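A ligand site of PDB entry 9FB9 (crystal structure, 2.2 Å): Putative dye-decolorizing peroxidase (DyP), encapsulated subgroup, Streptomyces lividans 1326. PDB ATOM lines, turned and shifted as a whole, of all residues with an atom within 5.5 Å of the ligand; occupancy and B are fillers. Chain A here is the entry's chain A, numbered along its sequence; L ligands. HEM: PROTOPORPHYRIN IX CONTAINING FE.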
ATOM      1  N   ASP A 146       3.586  19.493   9.262  1.00  0.00           N
ATOM      2  CA  ASP A 146       2.646  19.318  10.342  1.00  0.00           C
ATOM      3  C   ASP A 146       3.472  19.243  11.602  1.00  0.00           C
ATOM      4  O   ASP A 146       4.675  19.455  11.585  1.00  0.00           O
ATOM      5  CB  ASP A 146       1.717  18.140  10.101  1.00  0.00           C
ATOM      6  CG  ASP A 146       2.388  16.793   9.975  1.00  0.00           C
ATOM      7  OD1 ASP A 146       3.528  16.681  10.452  1.00  0.00           O
ATOM      8  OD2 ASP A 146       1.795  15.898   9.344  1.00  0.00           O
ATOM      9  N   LEU A 148       4.277  16.745  13.342  1.00  0.00           N
ATOM     10  CA  LEU A 148       5.298  15.722  13.386  1.00  0.00           C
ATOM     11  C   LEU A 148       6.517  16.047  12.525  1.00  0.00           C
ATOM     12  O   LEU A 148       7.446  15.245  12.463  1.00  0.00           O
ATOM     13  CB  LEU A 148       4.695  14.403  12.920  1.00  0.00           C
ATOM     14  CG  LEU A 148       3.483  13.934  13.730  1.00  0.00           C
ATOM     15  CD1 LEU A 148       3.044  12.609  13.143  1.00  0.00           C
ATOM     16  CD2 LEU A 148       3.743  13.776  15.219  1.00  0.00           C
ATOM     17  N   PHE A 150       6.656  16.525   9.166  1.00  0.00           N
ATOM     18  CA  PHE A 150       6.588  16.016   7.809  1.00  0.00           C
ATOM     19  C   PHE A 150       5.691  16.893   6.949  1.00  0.00           C
ATOM     20  O   PHE A 150       4.755  17.504   7.451  1.00  0.00           O
ATOM     21  CB  PHE A 150       5.994  14.621   7.795  1.00  0.00           C
ATOM     22  CG  PHE A 150       7.029  13.566   8.121  1.00  0.00           C
ATOM     23  CD1 PHE A 150       7.501  13.438   9.414  1.00  0.00           C
ATOM     24  CD2 PHE A 150       7.498  12.691   7.154  1.00  0.00           C
ATOM     25  CE1 PHE A 150       8.424  12.441   9.724  1.00  0.00           C
ATOM     26  CE2 PHE A 150       8.426  11.706   7.470  1.00  0.00           C
ATOM     27  CZ  PHE A 150       8.889  11.573   8.746  1.00  0.00           C
ATOM     28  N   VAL A 151       5.973  16.936   5.635  1.00  0.00           N
ATOM     29  CA  VAL A 151       5.172  17.728   4.714  1.00  0.00           C
ATOM     30  C   VAL A 151       3.838  16.998   4.602  1.00  0.00           C
ATOM     31  O   VAL A 151       3.811  15.746   4.446  1.00  0.00           O
ATOM     32  CB  VAL A 151       5.848  17.921   3.339  1.00  0.00           C
ATOM     33  CG1 VAL A 151       4.949  18.709   2.397  1.00  0.00           C
ATOM     34  CG2 VAL A 151       7.238  18.559   3.400  1.00  0.00           C
ATOM     35  N   ASP A 152       2.748  17.811   4.670  1.00  0.00           N
ATOM     36  CA  ASP A 152       1.377  17.345   4.833  1.00  0.00           C
ATOM     37  C   ASP A 152       0.483  17.982   3.764  1.00  0.00           C
ATOM     38  O   ASP A 152       0.238  19.200   3.762  1.00  0.00           O
ATOM     39  CB  ASP A 152       0.893  17.605   6.267  1.00  0.00           C
ATOM     40  CG  ASP A 152      -0.378  16.896   6.728  1.00  0.00           C
ATOM     41  OD1 ASP A 152      -1.328  16.860   5.900  1.00  0.00           O
ATOM     42  OD2 ASP A 152      -0.460  16.457   7.911  1.00  0.00           O
ATOM     43  N   GLY A 153      -0.011  17.140   2.851  1.00  0.00           N
ATOM     44  CA  GLY A 153      -0.822  17.613   1.733  1.00  0.00           C
ATOM     45  C   GLY A 153      -0.396  17.069   0.354  1.00  0.00           C
ATOM     46  O   GLY A 153      -1.161  17.226  -0.570  1.00  0.00           O
ATOM     47  N   THR A 154       0.780  16.425   0.220  1.00  0.00           N
ATOM     48  CA  THR A 154       1.543  16.301  -1.016  1.00  0.00           C
ATOM     49  C   THR A 154       0.783  15.496  -2.037  1.00  0.00           C
ATOM     50  O   THR A 154       0.721  15.891  -3.187  1.00  0.00           O
ATOM     51  CB  THR A 154       2.851  15.582  -0.745  1.00  0.00           C
ATOM     52  OG1 THR A 154       3.466  16.215   0.383  1.00  0.00           O
ATOM     53  CG2 THR A 154       3.765  15.583  -1.966  1.00  0.00           C
ATOM     54  N   GLU A 155       0.195  14.386  -1.586  1.00  0.00           N
ATOM     55  CA  GLU A 155      -0.542  13.470  -2.459  1.00  0.00           C
ATOM     56  C   GLU A 155      -2.049  13.759  -2.542  1.00  0.00           C
ATOM     57  O   GLU A 155      -2.825  12.956  -3.038  1.00  0.00           O
ATOM     58  CB  GLU A 155      -0.256  12.049  -1.982  1.00  0.00           C
ATOM     59  CG  GLU A 155       1.120  11.532  -2.384  1.00  0.00           C
ATOM     60  CD  GLU A 155       1.045  11.146  -3.832  1.00  0.00           C
ATOM     61  OE1 GLU A 155       0.315  10.154  -4.162  1.00  0.00           O
ATOM     62  OE2 GLU A 155       1.717  11.860  -4.598  1.00  0.00           O
ATOM     63  N   ASN A 156      -2.518  14.910  -2.097  1.00  0.00           N
ATOM     64  CA  ASN A 156      -3.910  15.254  -2.303  1.00  0.00           C
ATOM     65  C   ASN A 156      -4.215  15.333  -3.777  1.00  0.00           C
ATOM     66  O   ASN A 156      -3.382  15.850  -4.508  1.00  0.00           O
ATOM     67  CB  ASN A 156      -4.265  16.641  -1.805  1.00  0.00           C
ATOM     68  CG  ASN A 156      -4.822  16.575  -0.412  1.00  0.00           C
ATOM     69  OD1 ASN A 156      -5.600  15.664  -0.083  1.00  0.00           O
ATOM     70  ND2 ASN A 156      -4.423  17.521   0.412  1.00  0.00           N
ATOM     71  N   GLN A 184     -11.570  14.981  12.805  1.00  0.00           N
ATOM     72  CA  GLN A 184     -11.003  14.404  14.015  1.00  0.00           C
ATOM     73  C   GLN A 184      -9.934  15.353  14.566  1.00  0.00           C
ATOM     74  O   GLN A 184      -9.043  15.768  13.840  1.00  0.00           O
ATOM     75  CB  GLN A 184     -10.323  13.080  13.710  1.00  0.00           C
ATOM     76  CG  GLN A 184     -11.308  11.969  13.402  1.00  0.00           C
ATOM     77  CD  GLN A 184     -10.571  10.671  13.268  1.00  0.00           C
ATOM     78  OE1 GLN A 184      -9.720  10.558  12.372  1.00  0.00           O
ATOM     79  NE2 GLN A 184     -10.858   9.782  14.216  1.00  0.00           N
ATOM     80  N   TYR A 186      -6.696  15.505  16.632  1.00  0.00           N
ATOM     81  CA  TYR A 186      -5.662  14.597  17.118  1.00  0.00           C
ATOM     82  C   TYR A 186      -4.650  15.351  17.953  1.00  0.00           C
ATOM     83  O   TYR A 186      -4.229  16.431  17.553  1.00  0.00           O
ATOM     84  CB  TYR A 186      -4.850  13.957  16.006  1.00  0.00           C
ATOM     85  CG  TYR A 186      -5.551  12.808  15.335  1.00  0.00           C
ATOM     86  CD1 TYR A 186      -5.519  11.520  15.859  1.00  0.00           C
ATOM     87  CD2 TYR A 186      -6.270  13.019  14.186  1.00  0.00           C
ATOM     88  CE1 TYR A 186      -6.118  10.456  15.200  1.00  0.00           C
ATOM     89  CE2 TYR A 186      -6.915  11.970  13.546  1.00  0.00           C
ATOM     90  CZ  TYR A 186      -6.854  10.689  14.055  1.00  0.00           C
ATOM     91  OH  TYR A 186      -7.486   9.650  13.418  1.00  0.00           O
ATOM     92  N   HIS A 188      -0.739  14.953  19.652  1.00  0.00           N
ATOM     93  CA  HIS A 188       0.429  14.105  19.520  1.00  0.00           C
ATOM     94  C   HIS A 188       1.209  14.070  20.816  1.00  0.00           C
ATOM     95  O   HIS A 188       1.139  14.998  21.606  1.00  0.00           O
ATOM     96  CB  HIS A 188       1.306  14.595  18.379  1.00  0.00           C
ATOM     97  CG  HIS A 188       0.598  14.692  17.081  1.00  0.00           C
ATOM     98  ND1 HIS A 188       0.277  13.551  16.399  1.00  0.00           N
ATOM     99  CD2 HIS A 188       0.140  15.736  16.328  1.00  0.00           C
ATOM    100  CE1 HIS A 188      -0.299  13.913  15.239  1.00  0.00           C
ATOM    101  NE2 HIS A 188      -0.386  15.230  15.175  1.00  0.00           N
ATOM    102  N   ILE A 205       5.747   7.040   8.746  1.00  0.00           N
ATOM    103  CA  ILE A 205       4.956   7.798   7.805  1.00  0.00           C
ATOM    104  C   ILE A 205       4.921   7.068   6.470  1.00  0.00           C
ATOM    105  O   ILE A 205       3.843   6.952   5.889  1.00  0.00           O
ATOM    106  CB  ILE A 205       5.492   9.234   7.680  1.00  0.00           C
ATOM    107  CG1 ILE A 205       5.403   9.977   8.981  1.00  0.00           C
ATOM    108  CG2 ILE A 205       4.786  10.029   6.579  1.00  0.00           C
ATOM    109  CD1 ILE A 205       3.995  10.290   9.432  1.00  0.00           C
ATOM    110  N   ARG A 207       7.294   8.193   3.966  1.00  0.00           N
ATOM    111  CA  ARG A 207       7.986   9.101   3.059  1.00  0.00           C
ATOM    112  C   ARG A 207       9.228   9.658   3.737  1.00  0.00           C
ATOM    113  O   ARG A 207       9.358   9.562   4.948  1.00  0.00           O
ATOM    114  CB  ARG A 207       7.092  10.297   2.771  1.00  0.00           C
ATOM    115  CG  ARG A 207       5.665   9.925   2.422  1.00  0.00           C
ATOM    116  CD  ARG A 207       4.930  11.176   2.012  1.00  0.00           C
ATOM    117  NE  ARG A 207       5.429  11.820   0.781  1.00  0.00           N
ATOM    118  CZ  ARG A 207       5.017  11.520  -0.459  1.00  0.00           C
ATOM    119  NH1 ARG A 207       4.222  10.505  -0.753  1.00  0.00           N
ATOM    120  NH2 ARG A 207       5.363  12.343  -1.432  1.00  0.00           N
ATOM    121  N   ASP A 212      10.575  14.756   1.296  1.00  0.00           N
ATOM    122  CA  ASP A 212       9.194  14.410   1.020  1.00  0.00           C
ATOM    123  C   ASP A 212       9.036  13.509  -0.208  1.00  0.00           C
ATOM    124  O   ASP A 212       7.976  13.479  -0.817  1.00  0.00           O
ATOM    125  CB  ASP A 212       8.311  15.626   0.825  1.00  0.00           C
ATOM    126  CG  ASP A 212       6.811  15.386   0.898  1.00  0.00           C
ATOM    127  OD1 ASP A 212       6.377  14.445   1.702  1.00  0.00           O
ATOM    128  OD2 ASP A 212       6.114  16.246   0.240  1.00  0.00           O
ATOM    129  N   GLU A 214       8.468   9.689  -1.591  1.00  0.00           N
ATOM    130  CA  GLU A 214       7.942   8.426  -1.091  1.00  0.00           C
ATOM    131  C   GLU A 214       9.017   7.373  -0.897  1.00  0.00           C
ATOM    132  O   GLU A 214       9.949   7.268  -1.664  1.00  0.00           O
ATOM    133  CB  GLU A 214       6.957   7.912  -2.137  1.00  0.00           C
ATOM    134  CG  GLU A 214       5.959   6.900  -1.615  1.00  0.00           C
ATOM    135  CD  GLU A 214       4.688   6.721  -2.440  1.00  0.00           C
ATOM    136  OE1 GLU A 214       4.055   7.659  -3.021  1.00  0.00           O
ATOM    137  OE2 GLU A 214       4.315   5.547  -2.426  1.00  0.00           O
ATOM    138  N   HIS A 225       1.829   4.807   7.554  1.00  0.00           N
ATOM    139  CA  HIS A 225       0.608   5.565   7.369  1.00  0.00           C
ATOM    140  C   HIS A 225       0.210   5.612   5.890  1.00  0.00           C
ATOM    141  O   HIS A 225      -0.974   5.480   5.565  1.00  0.00           O
ATOM    142  CB  HIS A 225       0.743   6.969   7.948  1.00  0.00           C
ATOM    143  CG  HIS A 225      -0.476   7.841   7.816  1.00  0.00           C
ATOM    144  ND1 HIS A 225      -1.707   7.542   8.327  1.00  0.00           N
ATOM    145  CD2 HIS A 225      -0.619   9.046   7.238  1.00  0.00           C
ATOM    146  CE1 HIS A 225      -2.537   8.527   8.055  1.00  0.00           C
ATOM    147  NE2 HIS A 225      -1.905   9.444   7.377  1.00  0.00           N
ATOM    148  N   VAL A 226       1.206   5.779   5.011  1.00  0.00           N
ATOM    149  CA  VAL A 226       0.962   5.974   3.597  1.00  0.00           C
ATOM    150  C   VAL A 226       0.537   4.645   2.992  1.00  0.00           C
ATOM    151  O   VAL A 226      -0.226   4.613   2.041  1.00  0.00           O
ATOM    152  CB  VAL A 226       2.178   6.598   2.886  1.00  0.00           C
ATOM    153  CG1 VAL A 226       2.243   6.141   1.445  1.00  0.00           C
ATOM    154  CG2 VAL A 226       2.183   8.142   2.977  1.00  0.00           C
ATOM    155  N   THR A 229      -3.288   4.001   4.128  1.00  0.00           N
ATOM    156  CA  THR A 229      -4.293   4.902   3.607  1.00  0.00           C
ATOM    157  C   THR A 229      -4.265   4.928   2.078  1.00  0.00           C
ATOM    158  O   THR A 229      -4.941   5.768   1.471  1.00  0.00           O
ATOM    159  CB  THR A 229      -4.079   6.298   4.195  1.00  0.00           C
ATOM    160  OG1 THR A 229      -2.806   6.837   3.848  1.00  0.00           O
ATOM    161  CG2 THR A 229      -4.214   6.278   5.706  1.00  0.00           C
ATOM    162  N   SER A 230      -3.466   4.065   1.448  1.00  0.00           N
ATOM    163  CA  SER A 230      -3.551   3.836   0.016  1.00  0.00           C
ATOM    164  C   SER A 230      -4.548   2.716  -0.193  1.00  0.00           C
ATOM    165  O   SER A 230      -4.377   1.616   0.302  1.00  0.00           O
ATOM    166  CB  SER A 230      -2.210   3.497  -0.600  1.00  0.00           C
ATOM    167  OG  SER A 230      -1.373   4.627  -0.723  1.00  0.00           O
ATOM    168  N   ILE A 241      -9.271  10.917  -1.162  1.00  0.00           N
ATOM    169  CA  ILE A 241      -9.980  11.982  -0.449  1.00  0.00           C
ATOM    170  C   ILE A 241      -9.199  13.273  -0.535  1.00  0.00           C
ATOM    171  O   ILE A 241      -8.041  13.320  -0.934  1.00  0.00           O
ATOM    172  CB  ILE A 241     -10.201  11.605   1.022  1.00  0.00           C
ATOM    173  CG1 ILE A 241      -8.903  11.581   1.755  1.00  0.00           C
ATOM    174  CG2 ILE A 241     -10.938  10.276   1.118  1.00  0.00           C
ATOM    175  CD1 ILE A 241      -9.063  11.358   3.232  1.00  0.00           C
ATOM    176  N   ARG A 243      -7.751  16.233   1.835  1.00  0.00           N
ATOM    177  CA  ARG A 243      -7.428  16.572   3.210  1.00  0.00           C
ATOM    178  C   ARG A 243      -6.890  18.006   3.309  1.00  0.00           C
ATOM    179  O   ARG A 243      -6.355  18.526   2.357  1.00  0.00           O
ATOM    180  CB  ARG A 243      -6.325  15.682   3.772  1.00  0.00           C
ATOM    181  CG  ARG A 243      -6.675  14.210   3.829  1.00  0.00           C
ATOM    182  CD  ARG A 243      -5.431  13.409   4.147  1.00  0.00           C
ATOM    183  NE  ARG A 243      -4.685  13.292   2.896  1.00  0.00           N
ATOM    184  CZ  ARG A 243      -3.440  13.682   2.764  1.00  0.00           C
ATOM    185  NH1 ARG A 243      -2.741  14.049   3.842  1.00  0.00           N
ATOM    186  NH2 ARG A 243      -2.871  13.687   1.559  1.00  0.00           N
ATOM    187  N   ASN A 245      -5.279  19.176   6.577  1.00  0.00           N
ATOM    188  CA  ASN A 245      -4.878  19.070   7.977  1.00  0.00           C
ATOM    189  C   ASN A 245      -4.233  20.373   8.416  1.00  0.00           C
ATOM    190  O   ASN A 245      -3.449  20.946   7.661  1.00  0.00           O
ATOM    191  CB  ASN A 245      -3.956  17.877   8.229  1.00  0.00           C
ATOM    192  CG  ASN A 245      -4.610  16.580   7.817  1.00  0.00           C
ATOM    193  OD1 ASN A 245      -5.830  16.555   7.609  1.00  0.00           O
ATOM    194  ND2 ASN A 245      -3.852  15.487   7.684  1.00  0.00           N
ATOM    195  N   THR A 258      -2.814  17.994  15.419  1.00  0.00           N
ATOM    196  CA  THR A 258      -3.179  18.023  13.995  1.00  0.00           C
ATOM    197  C   THR A 258      -4.705  17.882  13.913  1.00  0.00           C
ATOM    198  O   THR A 258      -5.270  16.940  14.429  1.00  0.00           O
ATOM    199  CB  THR A 258      -2.388  16.930  13.250  1.00  0.00           C
ATOM    200  OG1 THR A 258      -1.011  17.320  13.067  1.00  0.00           O
ATOM    201  CG2 THR A 258      -3.103  16.598  11.958  1.00  0.00           C
ATOM    202  N   PHE A 260      -7.636  17.064  11.745  1.00  0.00           N
ATOM    203  CA  PHE A 260      -7.822  16.307  10.521  1.00  0.00           C
ATOM    204  C   PHE A 260      -9.189  16.630   9.936  1.00  0.00           C
ATOM    205  O   PHE A 260     -10.187  16.623  10.656  1.00  0.00           O
ATOM    206  CB  PHE A 260      -7.748  14.805  10.767  1.00  0.00           C
ATOM    207  CG  PHE A 260      -8.240  14.015   9.581  1.00  0.00           C
ATOM    208  CD1 PHE A 260      -7.427  13.772   8.506  1.00  0.00           C
ATOM    209  CD2 PHE A 260      -9.537  13.561   9.515  1.00  0.00           C
ATOM    210  CE1 PHE A 260      -7.894  13.062   7.404  1.00  0.00           C
ATOM    211  CE2 PHE A 260     -10.004  12.841   8.415  1.00  0.00           C
ATOM    212  CZ  PHE A 260      -9.179  12.574   7.373  1.00  0.00           C
ATOM    213  N   THR A 270     -13.530   7.503   3.102  1.00  0.00           N
ATOM    214  CA  THR A 270     -12.927   8.025   4.327  1.00  0.00           C
ATOM    215  C   THR A 270     -12.984   6.930   5.414  1.00  0.00           C
ATOM    216  O   THR A 270     -12.029   6.699   6.140  1.00  0.00           O
ATOM    217  CB  THR A 270     -13.589   9.353   4.791  1.00  0.00           C
ATOM    218  OG1 THR A 270     -13.748  10.555   4.008  1.00  0.00           O
ATOM    219  CG2 THR A 270     -12.754   9.977   5.873  1.00  0.00           C
ATOM    220  N   MET A 273     -10.447   3.954   5.042  1.00  0.00           N
ATOM    221  CA  MET A 273      -9.125   4.324   5.475  1.00  0.00           C
ATOM    222  C   MET A 273      -9.068   4.277   7.002  1.00  0.00           C
ATOM    223  O   MET A 273      -8.085   3.813   7.597  1.00  0.00           O
ATOM    224  CB  MET A 273      -8.778   5.727   4.962  1.00  0.00           C
ATOM    225  CG  MET A 273      -8.595   5.793   3.474  1.00  0.00           C
ATOM    226  SD  MET A 273      -8.611   7.510   2.895  1.00  0.00           S
ATOM    227  CE  MET A 273      -8.373   7.261   1.135  1.00  0.00           C
ATOM    228  N   LEU A 274     -10.124   4.747   7.659  1.00  0.00           N
ATOM    229  CA  LEU A 274     -10.128   4.785   9.106  1.00  0.00           C
ATOM    230  C   LEU A 274     -10.074   3.389   9.699  1.00  0.00           C
ATOM    231  O   LEU A 274      -9.355   3.182  10.678  1.00  0.00           O
ATOM    232  CB  LEU A 274     -11.351   5.551   9.574  1.00  0.00           C
ATOM    233  CG  LEU A 274     -11.232   7.077   9.581  1.00  0.00           C
ATOM    234  CD1 LEU A 274     -12.568   7.777   9.835  1.00  0.00           C
ATOM    235  CD2 LEU A 274     -10.265   7.505  10.655  1.00  0.00           C
ATOM    236  N   MET A 277      -6.681   2.047   9.503  1.00  0.00           N
ATOM    237  CA  MET A 277      -5.784   2.653  10.458  1.00  0.00           C
ATOM    238  C   MET A 277      -5.992   2.066  11.856  1.00  0.00           C
ATOM    239  O   MET A 277      -5.012   1.684  12.501  1.00  0.00           O
ATOM    240  CB  MET A 277      -5.983   4.165  10.494  1.00  0.00           C
ATOM    241  CG  MET A 277      -5.370   4.889   9.304  1.00  0.00           C
ATOM    242  SD  MET A 277      -5.943   6.601   9.225  1.00  0.00           S
ATOM    243  CE  MET A 277      -5.124   7.162  10.723  1.00  0.00           C
ATOM    244  N   ILE A 289       1.119   5.587  13.085  1.00  0.00           N
ATOM    245  CA  ILE A 289       1.015   6.992  13.427  1.00  0.00           C
ATOM    246  C   ILE A 289       0.152   7.170  14.675  1.00  0.00           C
ATOM    247  O   ILE A 289       0.268   8.181  15.370  1.00  0.00           O
ATOM    248  CB  ILE A 289       0.482   7.784  12.222  1.00  0.00           C
ATOM    249  CG1 ILE A 289       0.945   9.243  12.295  1.00  0.00           C
ATOM    250  CG2 ILE A 289      -1.040   7.680  12.118  1.00  0.00           C
ATOM    251  CD1 ILE A 289       0.527  10.135  11.127  1.00  0.00           C
ATOM    252  N   SER A 293      -0.454   9.583  18.202  1.00  0.00           N
ATOM    253  CA  SER A 293      -1.539  10.489  17.944  1.00  0.00           C
ATOM    254  C   SER A 293      -2.798   9.900  18.577  1.00  0.00           C
ATOM    255  O   SER A 293      -3.097   8.747  18.359  1.00  0.00           O
ATOM    256  CB  SER A 293      -1.697  10.712  16.471  1.00  0.00           C
ATOM    257  OG  SER A 293      -0.456  10.740  15.799  1.00  0.00           O
HETATM  258  CHA HEM L   1      -0.843  11.026   3.725  1.00  0.00           C
HETATM  259  CHB HEM L   1      -0.079  13.143   8.010  1.00  0.00           C
HETATM  260  CHC HEM L   1      -4.326  11.488   9.722  1.00  0.00           C
HETATM  261  CHD HEM L   1      -5.318  10.012   5.135  1.00  0.00           C
HETATM  262  C1A HEM L   1      -0.262  11.707   4.791  1.00  0.00           C
HETATM  263  C2A HEM L   1       1.065  12.204   4.720  1.00  0.00           C
HETATM  264  C3A HEM L   1       1.262  12.843   5.920  1.00  0.00           C
HETATM  265  C4A HEM L   1       0.093  12.691   6.731  1.00  0.00           C
HETATM  266  CMA HEM L   1       2.502  13.524   6.325  1.00  0.00           C
HETATM  267  CAA HEM L   1       2.036  12.055   3.561  1.00  0.00           C
HETATM  268  CBA HEM L   1       2.030  13.343   2.755  1.00  0.00           C
HETATM  269  CGA HEM L   1       0.683  13.547   2.141  1.00  0.00           C
HETATM  270  O1A HEM L   1      -0.034  14.378   2.717  1.00  0.00           O
HETATM  271  O2A HEM L   1       0.342  12.875   1.118  1.00  0.00           O
HETATM  272  C1B HEM L   1      -1.175  12.838   8.820  1.00  0.00           C
HETATM  273  C2B HEM L   1      -1.192  13.212  10.167  1.00  0.00           C
HETATM  274  C3B HEM L   1      -2.373  12.803  10.690  1.00  0.00           C
HETATM  275  C4B HEM L   1      -3.082  12.098   9.611  1.00  0.00           C
HETATM  276  CMB HEM L   1      -0.164  14.050  10.919  1.00  0.00           C
HETATM  277  CAB HEM L   1      -2.650  12.989  12.110  1.00  0.00           C
HETATM  278  CBB HEM L   1      -3.326  12.100  12.780  1.00  0.00           C
HETATM  279  C1C HEM L   1      -5.010  10.937   8.644  1.00  0.00           C
HETATM  280  C2C HEM L   1      -6.289  10.358   8.619  1.00  0.00           C
HETATM  281  C3C HEM L   1      -6.560   9.911   7.311  1.00  0.00           C
HETATM  282  C4C HEM L   1      -5.402  10.253   6.532  1.00  0.00           C
HETATM  283  CMC HEM L   1      -7.211  10.280   9.815  1.00  0.00           C
HETATM  284  CAC HEM L   1      -7.721   9.292   6.630  1.00  0.00           C
HETATM  285  CBC HEM L   1      -8.872   9.054   7.181  1.00  0.00           C
HETATM  286  C1D HEM L   1      -4.213  10.194   4.371  1.00  0.00           C
HETATM  287  C2D HEM L   1      -4.145   9.827   2.965  1.00  0.00           C
HETATM  288  C3D HEM L   1      -2.855  10.075   2.549  1.00  0.00           C
HETATM  289  C4D HEM L   1      -2.202  10.599   3.784  1.00  0.00           C
HETATM  290  CMD HEM L   1      -5.307   9.310   2.138  1.00  0.00           C
HETATM  291  CAD HEM L   1      -2.136   9.939   1.168  1.00  0.00           C
HETATM  292  CBD HEM L   1      -1.982   8.501   0.528  1.00  0.00           C
HETATM  293  CGD HEM L   1      -1.119   8.376  -0.754  1.00  0.00           C
HETATM  294  O1D HEM L   1      -1.511   7.929  -1.915  1.00  0.00           O
HETATM  295  O2D HEM L   1       0.059   8.759  -0.594  1.00  0.00           O
HETATM  296  NA  HEM L   1      -0.862  11.993   6.060  1.00  0.00           N
HETATM  297  NB  HEM L   1      -2.307  12.210   8.522  1.00  0.00           N
HETATM  298  NC  HEM L   1      -4.528  10.878   7.381  1.00  0.00           N
HETATM  299  ND  HEM L   1      -3.059  10.661   4.874  1.00  0.00           N
HETATM  300 FE   HEM L   1      -2.658  11.312   6.696  1.00  0.00          FE
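O1A of the ligand lies within hydrogen-bond range of N of Gly 153.
The backbone NH (N) of Glu 155 sits at hydrogen-bond distance from an oxygen (O2A) of the ligand (3.1 Å).
NE2 of His 225 binds FE of the ligand (2.1 Å).
O1A of the ligand is in salt-bridge range of NH1 of Arg 243 (2.9 Å).
O1A of the ligand is in hydrogen-bond range of N of Thr 154 (3.3 Å).
The backbone NH (N) of Tyr 186 lies within hydrogen-bond range of the backbone carbonyl oxygen (O) of Thr 258, 3.0 Å away.
The side-chain amide nitrogen (ND2) of Asn 156 sits close to the backbone carbonyl oxygen (O) of Gly 153 (3.4 Å).
OG1 of Thr 154 lies within hydrogen-bond range of OD2 of Asp 212 (2.7 Å).
The side-chain hydroxyl (OH) of Tyr 186 sits at hydrogen-bond distance from the side-chain amide oxygen (OE1) of Gln 184, 2.6 Å away.
OD2 of Asp 146 sits close to OD2 of Asp 152 (2.7 Å).
OD1 of Asp 212 lies within salt-bridge range of NE of Arg 207, 2.9 Å away.
The backbone NH (N) of His 225 sits at hydrogen-bond distance from the backbone carbonyl oxygen (O) of Ile 205, at 3.4 Å.
A ring nitrogen (NE2) of His 188 lies within hydrogen-bond range of the side-chain hydroxyl (OG1) of Thr 258.
Merely in contact with the ligand: Asp 146, Val 151, Asp 152, Phe 260, Tyr 186, Thr 229, Arg 207, Ser 230, Gln 184, Thr 258, Ile 289, Asn 245, Met 277, Met 273, Leu 274, Phe 150 and Val 226.
Hydrophobic or aromatic side chains within 4 Å of the ligand: Phe 150, Tyr 186, His 225, Val 226, Phe 260, Met 273, Leu 274, Met 277 and Ile 289.
22 residues have an atom within 4 Å of the ligand: Asp 146, Phe 150, Val 151, Asp 152, Gly 153, Thr 154, Glu 155, Gln 184, Tyr 186, Arg 207, His 225, Val 226, Thr 229, Ser 230, Arg 243, Asn 245, Thr 258, Phe 260, Met 273, Leu 274, Met 277 and Ile 289.
Along chain A the residues within 4 Å of the ligand span positions 146 to 289.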
